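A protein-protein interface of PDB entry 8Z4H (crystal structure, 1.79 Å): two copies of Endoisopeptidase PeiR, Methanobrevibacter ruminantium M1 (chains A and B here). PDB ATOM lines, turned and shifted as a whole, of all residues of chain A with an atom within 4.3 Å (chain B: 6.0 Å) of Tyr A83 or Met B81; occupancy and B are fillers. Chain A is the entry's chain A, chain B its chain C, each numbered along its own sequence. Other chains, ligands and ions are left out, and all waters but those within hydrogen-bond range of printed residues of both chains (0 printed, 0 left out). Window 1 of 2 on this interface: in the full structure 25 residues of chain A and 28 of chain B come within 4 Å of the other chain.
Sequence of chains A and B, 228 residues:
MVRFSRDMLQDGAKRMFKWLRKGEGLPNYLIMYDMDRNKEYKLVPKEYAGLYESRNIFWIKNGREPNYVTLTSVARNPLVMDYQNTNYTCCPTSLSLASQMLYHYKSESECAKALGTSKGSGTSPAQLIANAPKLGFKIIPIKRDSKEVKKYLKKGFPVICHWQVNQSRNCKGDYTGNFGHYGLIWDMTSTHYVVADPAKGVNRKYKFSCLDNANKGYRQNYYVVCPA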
ATOM      1  N   MET A  81      11.048  18.165 -12.694  1.00  0.00           N
ATOM      2  CA  MET A  81      12.407  18.085 -13.258  1.00  0.00           C
ATOM      3  C   MET A  81      13.434  18.348 -12.160  1.00  0.00           C
ATOM      4  O   MET A  81      13.266  19.246 -11.324  1.00  0.00           O
ATOM      5  CB  MET A  81      12.602  19.075 -14.407  1.00  0.00           C
ATOM      6  CG  MET A  81      13.992  18.947 -15.069  1.00  0.00           C
ATOM      7  SD  MET A  81      14.316  17.207 -15.553  1.00  0.00           S
ATOM      8  CE  MET A  81      16.088  17.244 -15.779  1.00  0.00           C
ATOM      9  N   ASP A  82      14.448  17.503 -12.106  1.00  0.00           N
ATOM     10  CA  ASP A  82      15.519  17.577 -11.121  1.00  0.00           C
ATOM     11  C   ASP A  82      16.823  17.350 -11.863  1.00  0.00           C
ATOM     12  O   ASP A  82      16.915  16.392 -12.625  1.00  0.00           O
ATOM     13  CB  ASP A  82      15.344  16.503 -10.052  1.00  0.00           C
ATOM     14  CG  ASP A  82      16.217  16.718  -8.864  1.00  0.00           C
ATOM     15  OD1 ASP A  82      16.786  17.810  -8.724  1.00  0.00           O
ATOM     16  OD2 ASP A  82      16.331  15.777  -8.047  1.00  0.00           O
ATOM     17  N   TYR A  83      17.785  18.250 -11.707  1.00  0.00           N
ATOM     18  CA  TYR A  83      19.027  18.182 -12.473  1.00  0.00           C
ATOM     19  C   TYR A  83      20.152  17.531 -11.670  1.00  0.00           C
ATOM     20  O   TYR A  83      20.151  17.519 -10.434  1.00  0.00           O
ATOM     21  CB  TYR A  83      19.447  19.584 -12.951  1.00  0.00           C
ATOM     22  CG  TYR A  83      18.446  20.259 -13.865  1.00  0.00           C
ATOM     23  CD1 TYR A  83      17.351  21.000 -13.361  1.00  0.00           C
ATOM     24  CD2 TYR A  83      18.568  20.132 -15.222  1.00  0.00           C
ATOM     25  CE1 TYR A  83      16.436  21.607 -14.225  1.00  0.00           C
ATOM     26  CE2 TYR A  83      17.673  20.708 -16.085  1.00  0.00           C
ATOM     27  CZ  TYR A  83      16.612  21.427 -15.616  1.00  0.00           C
ATOM     28  OH  TYR A  83      15.759  22.027 -16.590  1.00  0.00           O
ATOM     29  N   GLN A  84      21.108  16.930 -12.378  1.00  0.00           N
ATOM     30  CA  GLN A  84      22.256  16.370 -11.678  1.00  0.00           C
ATOM     31  C   GLN A  84      23.150  17.490 -11.164  1.00  0.00           C
ATOM     32  O   GLN A  84      23.378  18.484 -11.857  1.00  0.00           O
ATOM     33  CB  GLN A  84      23.029  15.426 -12.564  1.00  0.00           C
ATOM     34  CG  GLN A  84      23.680  16.062 -13.800  1.00  0.00           C
ATOM     35  CD  GLN A  84      24.267  15.008 -14.755  1.00  0.00           C
ATOM     36  OE1 GLN A  84      23.572  14.544 -15.660  1.00  0.00           O
ATOM     37  NE2 GLN A  84      25.543  14.655 -14.564  1.00  0.00           N
ATOM     38  N   ASN A  85      23.638  17.323  -9.929  1.00  0.00           N
ATOM     39  CA  ASN A  85      24.425  18.323  -9.202  1.00  0.00           C
ATOM     40  C   ASN A  85      25.906  18.299  -9.539  1.00  0.00           C
ATOM     41  O   ASN A  85      26.622  19.237  -9.167  1.00  0.00           O
ATOM     42  CB  ASN A  85      24.259  18.141  -7.681  1.00  0.00           C
ATOM     43  CG  ASN A  85      25.152  17.050  -7.107  1.00  0.00           C
ATOM     44  OD1 ASN A  85      25.299  15.969  -7.702  1.00  0.00           O
ATOM     45  ND2 ASN A  85      25.734  17.304  -5.922  1.00  0.00           N
ATOM     46  N   THR A  93      20.497  10.690  -9.974  1.00  0.00           N
ATOM     47  CA  THR A  93      19.449  11.667 -10.297  1.00  0.00           C
ATOM     48  C   THR A  93      18.299  10.997 -11.052  1.00  0.00           C
ATOM     49  O   THR A  93      17.113  11.209 -10.720  1.00  0.00           O
ATOM     50  CB  THR A  93      20.004  12.834 -11.118  1.00  0.00           C
ATOM     51  OG1 THR A  93      21.098  13.425 -10.423  1.00  0.00           O
ATOM     52  CG2 THR A  93      18.979  13.866 -11.304  1.00  0.00           C
ATOM     53  N   GLU A 108      18.448  12.988  -4.687  1.00  0.00           N
ATOM     54  CA  GLU A 108      19.625  12.657  -5.490  1.00  0.00           C
ATOM     55  C   GLU A 108      20.794  12.214  -4.623  1.00  0.00           C
ATOM     56  O   GLU A 108      21.461  11.217  -4.916  1.00  0.00           O
ATOM     57  CB  GLU A 108      20.021  13.875  -6.326  1.00  0.00           C
ATOM     58  CG  GLU A 108      21.467  13.821  -6.800  1.00  0.00           C
ATOM     59  CD  GLU A 108      21.688  14.829  -7.950  1.00  0.00           C
ATOM     60  OE1 GLU A 108      22.722  14.731  -8.629  1.00  0.00           O
ATOM     61  OE2 GLU A 108      20.760  15.695  -8.181  1.00  0.00           O
ATOM     62  N   PRO A 198      18.780  14.359 -16.899  1.00  0.00           N
ATOM     63  CA  PRO A 198      19.214  15.239 -15.800  1.00  0.00           C
ATOM     64  C   PRO A 198      20.272  16.277 -16.179  1.00  0.00           C
ATOM     65  O   PRO A 198      20.662  17.124 -15.343  1.00  0.00           O
ATOM     66  CB  PRO A 198      19.760  14.244 -14.764  1.00  0.00           C
ATOM     67  CG  PRO A 198      20.083  12.991 -15.551  1.00  0.00           C
ATOM     68  CD  PRO A 198      19.076  12.938 -16.640  1.00  0.00           C
ATOM     69  N   ILE B  57      22.478  25.170 -14.960  1.00  0.00           N
ATOM     70  CA  ILE B  57      22.083  23.963 -14.234  1.00  0.00           C
ATOM     71  C   ILE B  57      22.839  23.854 -12.911  1.00  0.00           C
ATOM     72  O   ILE B  57      22.228  23.754 -11.823  1.00  0.00           O
ATOM     73  CB  ILE B  57      22.283  22.709 -15.096  1.00  0.00           C
ATOM     74  CG1 ILE B  57      21.198  22.640 -16.157  1.00  0.00           C
ATOM     75  CG2 ILE B  57      22.268  21.408 -14.198  1.00  0.00           C
ATOM     76  CD1 ILE B  57      21.408  21.609 -17.236  1.00  0.00           C
ATOM     77  N   ILE B  60      21.967  26.812 -10.472  1.00  0.00           N
ATOM     78  CA  ILE B  60      20.639  26.738  -9.837  1.00  0.00           C
ATOM     79  C   ILE B  60      20.565  25.570  -8.867  1.00  0.00           C
ATOM     80  O   ILE B  60      20.082  25.718  -7.740  1.00  0.00           O
ATOM     81  CB  ILE B  60      19.528  26.638 -10.895  1.00  0.00           C
ATOM     82  CG1 ILE B  60      19.366  27.987 -11.609  1.00  0.00           C
ATOM     83  CG2 ILE B  60      18.173  26.114 -10.256  1.00  0.00           C
ATOM     84  CD1 ILE B  60      19.006  27.793 -13.084  1.00  0.00           C
ATOM     85  N   LYS B  61      21.108  24.409  -9.260  1.00  0.00           N
ATOM     86  CA  LYS B  61      21.014  23.235  -8.403  1.00  0.00           C
ATOM     87  C   LYS B  61      21.906  23.360  -7.162  1.00  0.00           C
ATOM     88  O   LYS B  61      21.516  22.948  -6.064  1.00  0.00           O
ATOM     89  CB  LYS B  61      21.337  21.991  -9.225  1.00  0.00           C
ATOM     90  CG  LYS B  61      21.741  20.730  -8.412  1.00  0.00           C
ATOM     91  CD  LYS B  61      20.532  19.851  -8.192  1.00  0.00           C
ATOM     92  CE  LYS B  61      20.767  18.817  -7.100  1.00  0.00           C
ATOM     93  NZ  LYS B  61      19.464  18.699  -6.302  1.00  0.00           N
ATOM     94  N   LEU B  79      18.060  28.552 -21.031  1.00  0.00           N
ATOM     95  CA  LEU B  79      17.051  28.497 -19.971  1.00  0.00           C
ATOM     96  C   LEU B  79      16.995  27.132 -19.266  1.00  0.00           C
ATOM     97  O   LEU B  79      16.899  26.069 -19.910  1.00  0.00           O
ATOM     98  CB  LEU B  79      15.682  28.837 -20.558  1.00  0.00           C
ATOM     99  CG  LEU B  79      14.540  28.880 -19.525  1.00  0.00           C
ATOM    100  CD1 LEU B  79      14.787  30.013 -18.503  1.00  0.00           C
ATOM    101  CD2 LEU B  79      13.220  29.055 -20.270  1.00  0.00           C
ATOM    102  N   VAL B  80      17.036  27.166 -17.930  1.00  0.00           N
ATOM    103  CA  VAL B  80      16.912  25.973 -17.084  1.00  0.00           C
ATOM    104  C   VAL B  80      15.712  26.133 -16.157  1.00  0.00           C
ATOM    105  O   VAL B  80      15.646  27.100 -15.379  1.00  0.00           O
ATOM    106  CB  VAL B  80      18.201  25.740 -16.270  1.00  0.00           C
ATOM    107  CG1 VAL B  80      18.028  24.547 -15.285  1.00  0.00           C
ATOM    108  CG2 VAL B  80      19.441  25.571 -17.228  1.00  0.00           C
ATOM    109  N   MET B  81      14.782  25.184 -16.200  1.00  0.00           N
ATOM    110  CA  MET B  81      13.604  25.307 -15.337  1.00  0.00           C
ATOM    111  C   MET B  81      14.040  25.499 -13.885  1.00  0.00           C
ATOM    112  O   MET B  81      14.872  24.751 -13.354  1.00  0.00           O
ATOM    113  CB  MET B  81      12.702  24.080 -15.444  1.00  0.00           C
ATOM    114  CG  MET B  81      11.262  24.259 -14.912  1.00  0.00           C
ATOM    115  SD  MET B  81      10.490  25.843 -15.118  1.00  0.00           S
ATOM    116  CE  MET B  81       9.209  25.806 -13.851  1.00  0.00           C
ATOM    117  N   ASP B  82      13.480  26.519 -13.265  1.00  0.00           N
ATOM    118  CA  ASP B  82      13.723  26.879 -11.880  1.00  0.00           C
ATOM    119  C   ASP B  82      12.347  27.089 -11.235  1.00  0.00           C
ATOM    120  O   ASP B  82      11.588  27.967 -11.660  1.00  0.00           O
ATOM    121  CB  ASP B  82      14.566  28.145 -11.813  1.00  0.00           C
ATOM    122  CG  ASP B  82      14.979  28.493 -10.403  1.00  0.00           C
ATOM    123  OD1 ASP B  82      14.915  27.603  -9.538  1.00  0.00           O
ATOM    124  OD2 ASP B  82      15.376  29.653 -10.143  1.00  0.00           O
ATOM    125  N   TYR B  83      12.044  26.327 -10.192  1.00  0.00           N
ATOM    126  CA  TYR B  83      10.727  26.357  -9.572  1.00  0.00           C
ATOM    127  C   TYR B  83      10.784  27.304  -8.401  1.00  0.00           C
ATOM    128  O   TYR B  83      11.835  27.463  -7.780  1.00  0.00           O
ATOM    129  CB  TYR B  83      10.297  24.949  -9.073  1.00  0.00           C
ATOM    130  CG  TYR B  83      10.179  23.896 -10.163  1.00  0.00           C
ATOM    131  CD1 TYR B  83      11.265  23.114 -10.525  1.00  0.00           C
ATOM    132  CD2 TYR B  83       8.991  23.678 -10.823  1.00  0.00           C
ATOM    133  CE1 TYR B  83      11.190  22.159 -11.518  1.00  0.00           C
ATOM    134  CE2 TYR B  83       8.909  22.695 -11.847  1.00  0.00           C
ATOM    135  CZ  TYR B  83      10.024  21.940 -12.175  1.00  0.00           C
ATOM    136  OH  TYR B  83       9.980  20.934 -13.168  1.00  0.00           O
ATOM    137  N   LEU B  97      14.273  33.597 -13.990  1.00  0.00           N
ATOM    138  CA  LEU B  97      14.265  32.923 -15.288  1.00  0.00           C
ATOM    139  C   LEU B  97      14.602  33.895 -16.441  1.00  0.00           C
ATOM    140  O   LEU B  97      15.379  33.561 -17.349  1.00  0.00           O
ATOM    141  CB  LEU B  97      12.897  32.274 -15.498  1.00  0.00           C
ATOM    142  CG  LEU B  97      12.540  31.083 -14.582  1.00  0.00           C
ATOM    143  CD1 LEU B  97      11.057  30.790 -14.604  1.00  0.00           C
ATOM    144  CD2 LEU B  97      13.335  29.834 -15.021  1.00  0.00           C
ATOM    145  N   GLN B 100      18.289  34.575 -16.785  1.00  0.00           N
ATOM    146  CA  GLN B 100      19.035  33.528 -17.498  1.00  0.00           C
ATOM    147  C   GLN B 100      19.101  33.832 -18.989  1.00  0.00           C
ATOM    148  O   GLN B 100      20.175  33.742 -19.618  1.00  0.00           O
ATOM    149  CB  GLN B 100      18.380  32.173 -17.312  1.00  0.00           C
ATOM    150  CG  GLN B 100      18.386  31.595 -15.939  1.00  0.00           C
ATOM    151  CD  GLN B 100      17.803  30.221 -15.969  1.00  0.00           C
ATOM    152  OE1 GLN B 100      18.196  29.407 -16.797  1.00  0.00           O
ATOM    153  NE2 GLN B 100      16.804  29.971 -15.121  1.00  0.00           N
ATOM    154  N   ALA B 196       7.064  29.625 -18.968  1.00  0.00           N
ATOM    155  CA  ALA B 196       7.796  28.961 -17.885  1.00  0.00           C
ATOM    156  C   ALA B 196       7.036  29.365 -16.625  1.00  0.00           C
ATOM    157  O   ALA B 196       7.111  30.510 -16.240  1.00  0.00           O
ATOM    158  CB  ALA B 196       9.215  29.444 -17.850  1.00  0.00           C
ATOM    159  N   ASP B 197       6.239  28.449 -16.096  1.00  0.00           N
ATOM    160  CA  ASP B 197       5.456  28.701 -14.899  1.00  0.00           C
ATOM    161  C   ASP B 197       6.175  28.119 -13.673  1.00  0.00           C
ATOM    162  O   ASP B 197       6.253  26.897 -13.533  1.00  0.00           O
ATOM    163  CB  ASP B 197       4.041  28.106 -15.078  1.00  0.00           C
ATOM    164  CG  ASP B 197       3.155  28.276 -13.855  1.00  0.00           C
ATOM    165  OD1 ASP B 197       3.665  28.697 -12.781  1.00  0.00           O
ATOM    166  OD2 ASP B 197       1.930  27.987 -13.980  1.00  0.00           O
ATOM    167  N   PRO B 198       6.632  28.947 -12.736  1.00  0.00           N
ATOM    168  CA  PRO B 198       7.464  28.450 -11.625  1.00  0.00           C
ATOM    169  C   PRO B 198       6.771  27.486 -10.670  1.00  0.00           C
ATOM    170  O   PRO B 198       7.458  26.948  -9.783  1.00  0.00           O
ATOM    171  CB  PRO B 198       7.846  29.730 -10.868  1.00  0.00           C
ATOM    172  CG  PRO B 198       7.551  30.864 -11.827  1.00  0.00           C
ATOM    173  CD  PRO B 198       6.363  30.399 -12.632  1.00  0.00           C
ATOM    174  N   ALA B 199       5.443  27.287 -10.774  1.00  0.00           N
ATOM    175  CA  ALA B 199       4.729  26.296  -9.984  1.00  0.00           C
ATOM    176  C   ALA B 199       4.310  25.061 -10.798  1.00  0.00           C
ATOM    177  O   ALA B 199       3.648  24.162 -10.238  1.00  0.00           O
ATOM    178  CB  ALA B 199       3.486  26.968  -9.350  1.00  0.00           C
ATOM    179  N   LYS B 200       4.599  25.012 -12.100  1.00  0.00           N
ATOM    180  CA  LYS B 200       4.080  23.957 -12.968  1.00  0.00           C
ATOM    181  C   LYS B 200       5.118  23.370 -13.937  1.00  0.00           C
ATOM    182  O   LYS B 200       5.229  22.138 -14.028  1.00  0.00           O
ATOM    183  CB  LYS B 200       2.878  24.454 -13.768  1.00  0.00           C
ATOM    184  CG  LYS B 200       1.511  24.440 -12.985  1.00  0.00           C
ATOM    185  CD  LYS B 200       1.156  23.041 -12.420  1.00  0.00           C
ATOM    186  CE  LYS B 200       0.692  22.105 -13.513  1.00  0.00           C
ATOM    187  NZ  LYS B 200       0.887  20.661 -13.184  1.00  0.00           N
ATOM    188  N   GLY B 201       5.839  24.196 -14.699  1.00  0.00           N
ATOM    189  CA  GLY B 201       6.785  23.641 -15.659  1.00  0.00           C
ATOM    190  C   GLY B 201       7.261  24.672 -16.663  1.00  0.00           C
ATOM    191  O   GLY B 201       6.760  25.811 -16.729  1.00  0.00           O
ATOM    192  N   VAL B 202       8.196  24.227 -17.501  1.00  0.00           N
ATOM    193  CA  VAL B 202       8.925  25.164 -18.361  1.00  0.00           C
ATOM    194  C   VAL B 202       8.214  25.508 -19.674  1.00  0.00           C
ATOM    195  O   VAL B 202       8.565  26.515 -20.295  1.00  0.00           O
ATOM    196  CB  VAL B 202      10.346  24.631 -18.665  1.00  0.00           C
ATOM    197  CG1 VAL B 202      10.297  23.486 -19.676  1.00  0.00           C
ATOM    198  CG2 VAL B 202      11.245  25.762 -19.171  1.00  0.00           C
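The backbone carbonyl oxygen (O) of Pro A198 lies within hydrogen-bond range of the backbone NH (N) of Gln A84, 3.0 Å away.
SD of Met B81 sits close to N of Val B202 (3.7 Å).
The side-chain carboxylate of Glu A108 lies within hydrogen-bond range of the side-chain hydroxyl of Thr A93 (2.7 Å).
N of Val B80 is in hydrogen-bond range of OE1 of Gln B100 (2.8 Å).
OD1 of Asn A85 lies close to OE1 of Glu A108.
OE2 of Glu A108 lies within salt-bridge range of NZ of Lys B61 (3.8 Å).
N of Met B81 lies within hydrogen-bond range of OH of Tyr A83 (3.3 Å).
The side-chain amino group (NZ) of Lys B61 lies within salt-bridge range of the side-chain carboxylate (OD1) of Asp A82, 3.7 Å away.
N of Met A81 lies within hydrogen-bond range of OH of Tyr B83.
Of the 17 printed residues of chain B, 5 touch a printed residue of chain A.
Among the printed residues, Asp or Glu carboxylates within 4 Å of a Lys or Arg side-chain nitrogen of the other chain: Asp A82 with Lys B61 (3.7 Å) and Glu A108 with Lys B61 (3.8 Å).
Of the printed residues of chain B, Glu A108 touches Lys B61.
Printed residues of chain A within 4 Å of Ile B57: Tyr A83 (3.6 Å) and Gln A84 (3.9 Å).
Of the printed residues of chain A, Lys B61 touches Asp A82 (3.7 Å), Tyr A83 (3.3 Å), Asn A85 (3.6 Å) and Glu A108 (3.3 Å).
Of chain A, only Tyr A83 (3.3 Å) comes within 4 Å of Met B81.
Of the printed residues of chain A, Tyr B83 touches Met A81 (3.0 Å).
Ala B199 touches none of the printed residues of chain A.
The nearest residue of chain B that does not touch Tyr A83 is Leu B79 (5.4 Å).
The nearest printed residue of chain A that does not touch Met B81 is Met A81 (5.1 Å).
The nearest printed residue of chain B that does not touch Asn A85 is Ile B57 (6.1 Å).
Met A81 touches Tyr B83, and with the chains exchanged Tyr A83 touches Met B81.
4 positions are printed for both chains.
Tyr A83 touches Ile B57.
Tyr A83 touches Lys B61.
Tyr A83 touches Val B80 (CZ to CG1, 3.4 Å).
O of Gln A84 touches CG2 of Ile B57, at 3.9 Å.
CB of Asn A85 touches CE of Lys B61, at 3.6 Å.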
